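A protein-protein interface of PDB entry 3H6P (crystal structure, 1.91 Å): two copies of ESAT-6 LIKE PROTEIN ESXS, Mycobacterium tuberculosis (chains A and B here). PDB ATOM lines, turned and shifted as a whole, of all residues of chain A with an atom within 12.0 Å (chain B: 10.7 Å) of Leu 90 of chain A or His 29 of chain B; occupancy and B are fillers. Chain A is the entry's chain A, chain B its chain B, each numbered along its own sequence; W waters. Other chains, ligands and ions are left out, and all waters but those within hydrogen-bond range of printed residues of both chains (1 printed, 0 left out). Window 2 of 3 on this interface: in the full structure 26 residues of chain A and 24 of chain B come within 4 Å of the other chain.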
ATOM      1  N   THR A  81     -31.395 -32.481   2.314  1.00  0.00           N
ATOM      2  CA  THR A  81     -30.982 -32.390   3.719  1.00  0.00           C
ATOM      3  C   THR A  81     -29.549 -32.865   3.924  1.00  0.00           C
ATOM      4  O   THR A  81     -28.767 -32.211   4.630  1.00  0.00           O
ATOM      5  CB  THR A  81     -31.931 -33.203   4.629  1.00  0.00           C
ATOM      6  OG1 THR A  81     -33.260 -32.658   4.535  1.00  0.00           O
ATOM      7  CG2 THR A  81     -31.457 -33.144   6.073  1.00  0.00           C
ATOM      8  N   LEU A  82     -29.197 -33.985   3.288  1.00  0.00           N
ATOM      9  CA  LEU A  82     -27.843 -34.531   3.433  1.00  0.00           C
ATOM     10  C   LEU A  82     -26.777 -33.674   2.734  1.00  0.00           C
ATOM     11  O   LEU A  82     -25.627 -33.654   3.175  1.00  0.00           O
ATOM     12  CB  LEU A  82     -27.795 -35.980   2.943  1.00  0.00           C
ATOM     13  CG  LEU A  82     -28.555 -36.932   3.850  1.00  0.00           C
ATOM     14  CD1 LEU A  82     -28.878 -38.240   3.134  1.00  0.00           C
ATOM     15  CD2 LEU A  82     -27.749 -37.200   5.129  1.00  0.00           C
ATOM     16  N   LEU A  83     -27.129 -33.011   1.625  1.00  0.00           N
ATOM     17  CA  LEU A  83     -26.189 -32.106   0.969  1.00  0.00           C
ATOM     18  C   LEU A  83     -25.895 -30.910   1.874  1.00  0.00           C
ATOM     19  O   LEU A  83     -24.770 -30.425   1.943  1.00  0.00           O
ATOM     20  CB  LEU A  83     -26.748 -31.592  -0.371  1.00  0.00           C
ATOM     21  CG  LEU A  83     -26.650 -32.490  -1.584  1.00  0.00           C
ATOM     22  CD1 LEU A  83     -27.383 -31.871  -2.783  1.00  0.00           C
ATOM     23  CD2 LEU A  83     -25.158 -32.744  -1.865  1.00  0.00           C
ATOM     24  N   ASP A  84     -26.917 -30.403   2.550  1.00  0.00           N
ATOM     25  CA  ASP A  84     -26.700 -29.305   3.503  1.00  0.00           C
ATOM     26  C   ASP A  84     -25.792 -29.718   4.645  1.00  0.00           C
ATOM     27  O   ASP A  84     -24.895 -28.958   5.027  1.00  0.00           O
ATOM     28  CB  ASP A  84     -28.017 -28.777   4.046  1.00  0.00           C
ATOM     29  CG  ASP A  84     -28.823 -28.066   2.998  1.00  0.00           C
ATOM     30  OD1 ASP A  84     -28.248 -27.684   1.960  1.00  0.00           O
ATOM     31  OD2 ASP A  84     -30.051 -27.915   3.205  1.00  0.00           O
ATOM     32  N   ILE A  85     -26.003 -30.915   5.182  1.00  0.00           N
ATOM     33  CA  ILE A  85     -25.130 -31.443   6.222  1.00  0.00           C
ATOM     34  C   ILE A  85     -23.678 -31.552   5.743  1.00  0.00           C
ATOM     35  O   ILE A  85     -22.767 -31.177   6.460  1.00  0.00           O
ATOM     36  CB  ILE A  85     -25.621 -32.827   6.787  1.00  0.00           C
ATOM     37  CG1 ILE A  85     -26.936 -32.659   7.541  1.00  0.00           C
ATOM     38  CG2 ILE A  85     -24.566 -33.417   7.745  1.00  0.00           C
ATOM     39  CD1 ILE A  85     -27.653 -33.970   7.867  1.00  0.00           C
ATOM     40  N   ALA A  86     -23.476 -32.042   4.526  1.00  0.00           N
ATOM     41  CA  ALA A  86     -22.154 -32.136   3.948  1.00  0.00           C
ATOM     42  C   ALA A  86     -21.528 -30.757   3.864  1.00  0.00           C
ATOM     43  O   ALA A  86     -20.402 -30.581   4.300  1.00  0.00           O
ATOM     44  CB  ALA A  86     -22.205 -32.803   2.577  1.00  0.00           C
ATOM     45  N   GLN A  87     -22.272 -29.777   3.356  1.00  0.00           N
ATOM     46  CA  GLN A  87     -21.779 -28.411   3.217  1.00  0.00           C
ATOM     47  C   GLN A  87     -21.349 -27.811   4.561  1.00  0.00           C
ATOM     48  O   GLN A  87     -20.271 -27.195   4.654  1.00  0.00           O
ATOM     49  CB  GLN A  87     -22.828 -27.505   2.542  1.00  0.00           C
ATOM     50  CG  GLN A  87     -22.249 -26.136   2.178  1.00  0.00           C
ATOM     51  CD  GLN A  87     -23.242 -25.148   1.604  1.00  0.00           C
ATOM     52  OE1 GLN A  87     -23.025 -23.917   1.696  1.00  0.00           O
ATOM     53  NE2 GLN A  87     -24.278 -25.645   0.964  1.00  0.00           N
ATOM     54  N   ALA A  88     -22.185 -28.008   5.592  1.00  0.00           N
ATOM     55  CA  ALA A  88     -21.886 -27.556   6.974  1.00  0.00           C
ATOM     56  C   ALA A  88     -20.611 -28.175   7.529  1.00  0.00           C
ATOM     57  O   ALA A  88     -19.977 -27.598   8.407  1.00  0.00           O
ATOM     58  CB  ALA A  88     -23.066 -27.876   7.927  1.00  0.00           C
ATOM     59  N   ASN A  89     -20.263 -29.366   7.057  1.00  0.00           N
ATOM     60  CA  ASN A  89     -19.097 -30.088   7.564  1.00  0.00           C
ATOM     61  C   ASN A  89     -17.858 -29.925   6.685  1.00  0.00           C
ATOM     62  O   ASN A  89     -16.872 -30.663   6.849  1.00  0.00           O
ATOM     63  CB  ASN A  89     -19.448 -31.563   7.764  1.00  0.00           C
ATOM     64  CG  ASN A  89     -20.217 -31.790   9.037  1.00  0.00           C
ATOM     65  OD1 ASN A  89     -19.650 -31.755  10.109  1.00  0.00           O
ATOM     66  ND2 ASN A  89     -21.513 -31.985   8.931  1.00  0.00           N
ATOM     67  N   LEU A  90     -17.899 -28.978   5.746  1.00  0.00           N
ATOM     68  CA  LEU A  90     -16.729 -28.666   4.927  1.00  0.00           C
ATOM     69  C   LEU A  90     -15.974 -27.509   5.570  1.00  0.00           C
ATOM     70  O   LEU A  90     -14.744 -27.542   5.664  1.00  0.00           O
ATOM     71  CB  LEU A  90     -17.120 -28.282   3.495  1.00  0.00           C
ATOM     72  CG  LEU A  90     -17.762 -29.314   2.574  1.00  0.00           C
ATOM     73  CD1 LEU A  90     -17.970 -28.692   1.193  1.00  0.00           C
ATOM     74  CD2 LEU A  90     -16.944 -30.599   2.461  1.00  0.00           C
ATOM     75  N   SER B  28     -11.902 -27.888  -3.840  1.00  0.00           N
ATOM     76  CA  SER B  28     -12.535 -28.353  -2.566  1.00  0.00           C
ATOM     77  C   SER B  28     -13.968 -27.842  -2.410  1.00  0.00           C
ATOM     78  O   SER B  28     -14.924 -28.573  -2.674  1.00  0.00           O
ATOM     79  CB  SER B  28     -11.690 -27.923  -1.354  1.00  0.00           C
ATOM     80  OG  SER B  28     -12.481 -27.880  -0.172  1.00  0.00           O
ATOM     81  N   HIS B  29     -14.101 -26.586  -1.976  1.00  0.00           N
ATOM     82  CA  HIS B  29     -15.406 -26.021  -1.613  1.00  0.00           C
ATOM     83  C   HIS B  29     -16.198 -25.590  -2.844  1.00  0.00           C
ATOM     84  O   HIS B  29     -17.423 -25.762  -2.888  1.00  0.00           O
ATOM     85  CB  HIS B  29     -15.229 -24.846  -0.642  1.00  0.00           C
ATOM     86  CG  HIS B  29     -14.535 -25.224   0.632  1.00  0.00           C
ATOM     87  ND1 HIS B  29     -13.464 -24.517   1.139  1.00  0.00           N
ATOM     88  CD2 HIS B  29     -14.741 -26.257   1.484  1.00  0.00           C
ATOM     89  CE1 HIS B  29     -13.054 -25.087   2.261  1.00  0.00           C
ATOM     90  NE2 HIS B  29     -13.811 -26.146   2.492  1.00  0.00           N
ATOM     91  N   THR B  30     -15.501 -25.034  -3.837  1.00  0.00           N
ATOM     92  CA  THR B  30     -16.146 -24.666  -5.098  1.00  0.00           C
ATOM     93  C   THR B  30     -16.395 -25.933  -5.906  1.00  0.00           C
ATOM     94  O   THR B  30     -17.365 -26.001  -6.672  1.00  0.00           O
ATOM     95  CB  THR B  30     -15.342 -23.620  -5.922  1.00  0.00           C
ATOM     96  OG1 THR B  30     -14.268 -24.253  -6.636  1.00  0.00           O
ATOM     97  CG2 THR B  30     -14.781 -22.519  -5.014  1.00  0.00           C
ATOM     98  N   ALA B  31     -15.526 -26.933  -5.713  1.00  0.00           N
ATOM     99  CA  ALA B  31     -15.759 -28.270  -6.262  1.00  0.00           C
ATOM    100  C   ALA B  31     -17.008 -28.906  -5.652  1.00  0.00           C
ATOM    101  O   ALA B  31     -17.834 -29.422  -6.386  1.00  0.00           O
ATOM    102  CB  ALA B  31     -14.573 -29.158  -6.032  1.00  0.00           C
ATOM    103  N   PHE B  32     -17.139 -28.878  -4.317  1.00  0.00           N
ATOM    104  CA  PHE B  32     -18.382 -29.369  -3.681  1.00  0.00           C
ATOM    105  C   PHE B  32     -19.572 -28.591  -4.187  1.00  0.00           C
ATOM    106  O   PHE B  32     -20.603 -29.174  -4.524  1.00  0.00           O
ATOM    107  CB  PHE B  32     -18.350 -29.301  -2.138  1.00  0.00           C
ATOM    108  CG  PHE B  32     -19.709 -29.529  -1.502  1.00  0.00           C
ATOM    109  CD1 PHE B  32     -20.124 -30.812  -1.160  1.00  0.00           C
ATOM    110  CD2 PHE B  32     -20.589 -28.459  -1.291  1.00  0.00           C
ATOM    111  CE1 PHE B  32     -21.411 -31.036  -0.628  1.00  0.00           C
ATOM    112  CE2 PHE B  32     -21.878 -28.671  -0.743  1.00  0.00           C
ATOM    113  CZ  PHE B  32     -22.282 -29.958  -0.418  1.00  0.00           C
ATOM    114  N   ALA B  33     -19.458 -27.268  -4.243  1.00  0.00           N
ATOM    115  CA  ALA B  33     -20.592 -26.447  -4.708  1.00  0.00           C
ATOM    116  C   ALA B  33     -21.042 -26.841  -6.114  1.00  0.00           C
ATOM    117  O   ALA B  33     -22.238 -26.946  -6.396  1.00  0.00           O
ATOM    118  CB  ALA B  33     -20.222 -24.981  -4.667  1.00  0.00           C
ATOM    119  N   ALA B  34     -20.075 -27.055  -6.996  1.00  0.00           N
ATOM    120  CA  ALA B  34     -20.350 -27.462  -8.364  1.00  0.00           C
ATOM    121  C   ALA B  34     -21.159 -28.756  -8.381  1.00  0.00           C
ATOM    122  O   ALA B  34     -22.160 -28.884  -9.097  1.00  0.00           O
ATOM    123  CB  ALA B  34     -19.033 -27.642  -9.118  1.00  0.00           C
ATOM    124  N   LYS B  35     -20.724 -29.725  -7.584  1.00  0.00           N
ATOM    125  CA  LYS B  35     -21.366 -31.059  -7.584  1.00  0.00           C
ATOM    126  C   LYS B  35     -22.715 -31.032  -6.902  1.00  0.00           C
ATOM    127  O   LYS B  35     -23.641 -31.676  -7.358  1.00  0.00           O
ATOM    128  CB  LYS B  35     -20.479 -32.081  -6.872  1.00  0.00           C
ATOM    129  CG  LYS B  35     -19.201 -32.365  -7.591  1.00  0.00           C
ATOM    130  CD  LYS B  35     -18.288 -33.222  -6.735  1.00  0.00           C
ATOM    131  CE  LYS B  35     -16.978 -33.499  -7.445  1.00  0.00           C
ATOM    132  NZ  LYS B  35     -16.011 -32.423  -7.154  1.00  0.00           N
ATOM    133  N   ALA B  36     -22.812 -30.307  -5.787  1.00  0.00           N
ATOM    134  CA  ALA B  36     -24.102 -30.188  -5.105  1.00  0.00           C
ATOM    135  C   ALA B  36     -25.147 -29.540  -6.025  1.00  0.00           C
ATOM    136  O   ALA B  36     -26.284 -30.014  -6.130  1.00  0.00           O
ATOM    137  CB  ALA B  36     -23.931 -29.390  -3.765  1.00  0.00           C
ATOM    138  N   GLY B  37     -24.747 -28.480  -6.716  1.00  0.00           N
ATOM    139  CA  GLY B  37     -25.634 -27.773  -7.632  1.00  0.00           C
ATOM    140  C   GLY B  37     -26.100 -28.644  -8.777  1.00  0.00           C
ATOM    141  O   GLY B  37     -27.279 -28.631  -9.138  1.00  0.00           O
ATOM    142  N   ARG B  40     -28.608 -31.249  -7.524  1.00  0.00           N
ATOM    143  CA  ARG B  40     -29.956 -30.662  -7.351  1.00  0.00           C
ATOM    144  C   ARG B  40     -30.628 -30.423  -8.704  1.00  0.00           C
ATOM    145  O   ARG B  40     -31.794 -30.746  -8.897  1.00  0.00           O
ATOM    146  CB  ARG B  40     -29.878 -29.363  -6.555  1.00  0.00           C
ATOM    147  CG  ARG B  40     -29.541 -29.607  -5.095  1.00  0.00           C
ATOM    148  CD  ARG B  40     -29.365 -28.324  -4.340  1.00  0.00           C
ATOM    149  NE  ARG B  40     -29.553 -28.546  -2.905  1.00  0.00           N
ATOM    150  CZ  ARG B  40     -28.604 -28.468  -1.975  1.00  0.00           C
ATOM    151  NH1 ARG B  40     -27.357 -28.110  -2.271  1.00  0.00           N
ATOM    152  NH2 ARG B  40     -28.927 -28.703  -0.716  1.00  0.00           N
HETATM  153  O   HOH W   1     -25.805 -27.616   0.278  1.00  0.00           O
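OG of Ser 28 of chain B sits close to NE2 of His 29 of chain B, 3.4 Å away.
Hydrophobic or aromatic side chains of chain B within 4 Å of the printed part of chain A: His 29 and Phe 32. Of the 10 printed residues of chain A, 5 touch a printed residue of chain B. Hydrophobic or aromatic side chains of chain A within 4 Å of the printed part of chain B: Leu 83, Ala 86 and Leu 90. Among the printed residues, 8 pairs touch across the chains.
CZ of Phe 32 of chain B touches O of Leu 83 of chain A, at 3.5 Å. Leu 83 of chain A touches Ala 36 of chain B (CD1 to O, 3.98 Å). Arg 40 of chain B touches Leu 83 of chain A. CE1 of Phe 32 of chain B touches CB of Ala 86 of chain A, at 3.7 Å. Gln 87 of chain A touches Phe 32 of chain B. Leu 90 of chain A touches His 29 of chain B. Phe 32 of chain B touches Leu 90 of chain A (CG to CD1, 3.3 Å).
Water W1 lies within hydrogen-bond range of NE2 of Gln 87 of chain A, OD1 of Asp 84 of chain A, NH1 of Arg 40 of chain B and O of Leu 83 of chain A.
OD1 of Asp 84 of chain A lies within salt-bridge range of NH2 of Arg 40 of chain B.
Of the printed residues of chain B, Leu 83 of chain A touches Phe 32, Ala 36 and Arg 40. Of the printed residues of chain B, Asp 84 of chain A touches Arg 40 (2.9 Å). Ala 86 of chain A touches just one residue of chain B: Phe 32 (3.7 Å). No residue of chain B comes within 4 Å of Ala 88 of chain A. No residue of chain B comes within 4 Å of Asn 89 of chain A. Leu 90 of chain A touches two residues of chain B. No residue of chain A comes within 4 Å of Ser 28 of chain B. Thr 30 of chain B touches none of the printed residues of chain A. Of chain A, only Leu 83, Ala 86, Gln 87 and Leu 90 come within 4 Å of Phe 32 of chain B. Ala 33 of chain B touches none of the printed residues of chain A. Printed residues of chain A within 4 Å of Arg 40 of chain B: Leu 83 (3.6 Å) and Asp 84 (2.9 Å). The nearest residue of chain A that does not touch His 29 of chain B is Gln 87 of chain A (6.4 Å). The nearest printed residue of chain A that does not touch Arg 40 of chain B is Gln 87 of chain A (5.1 Å).
No position is printed for both chains.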
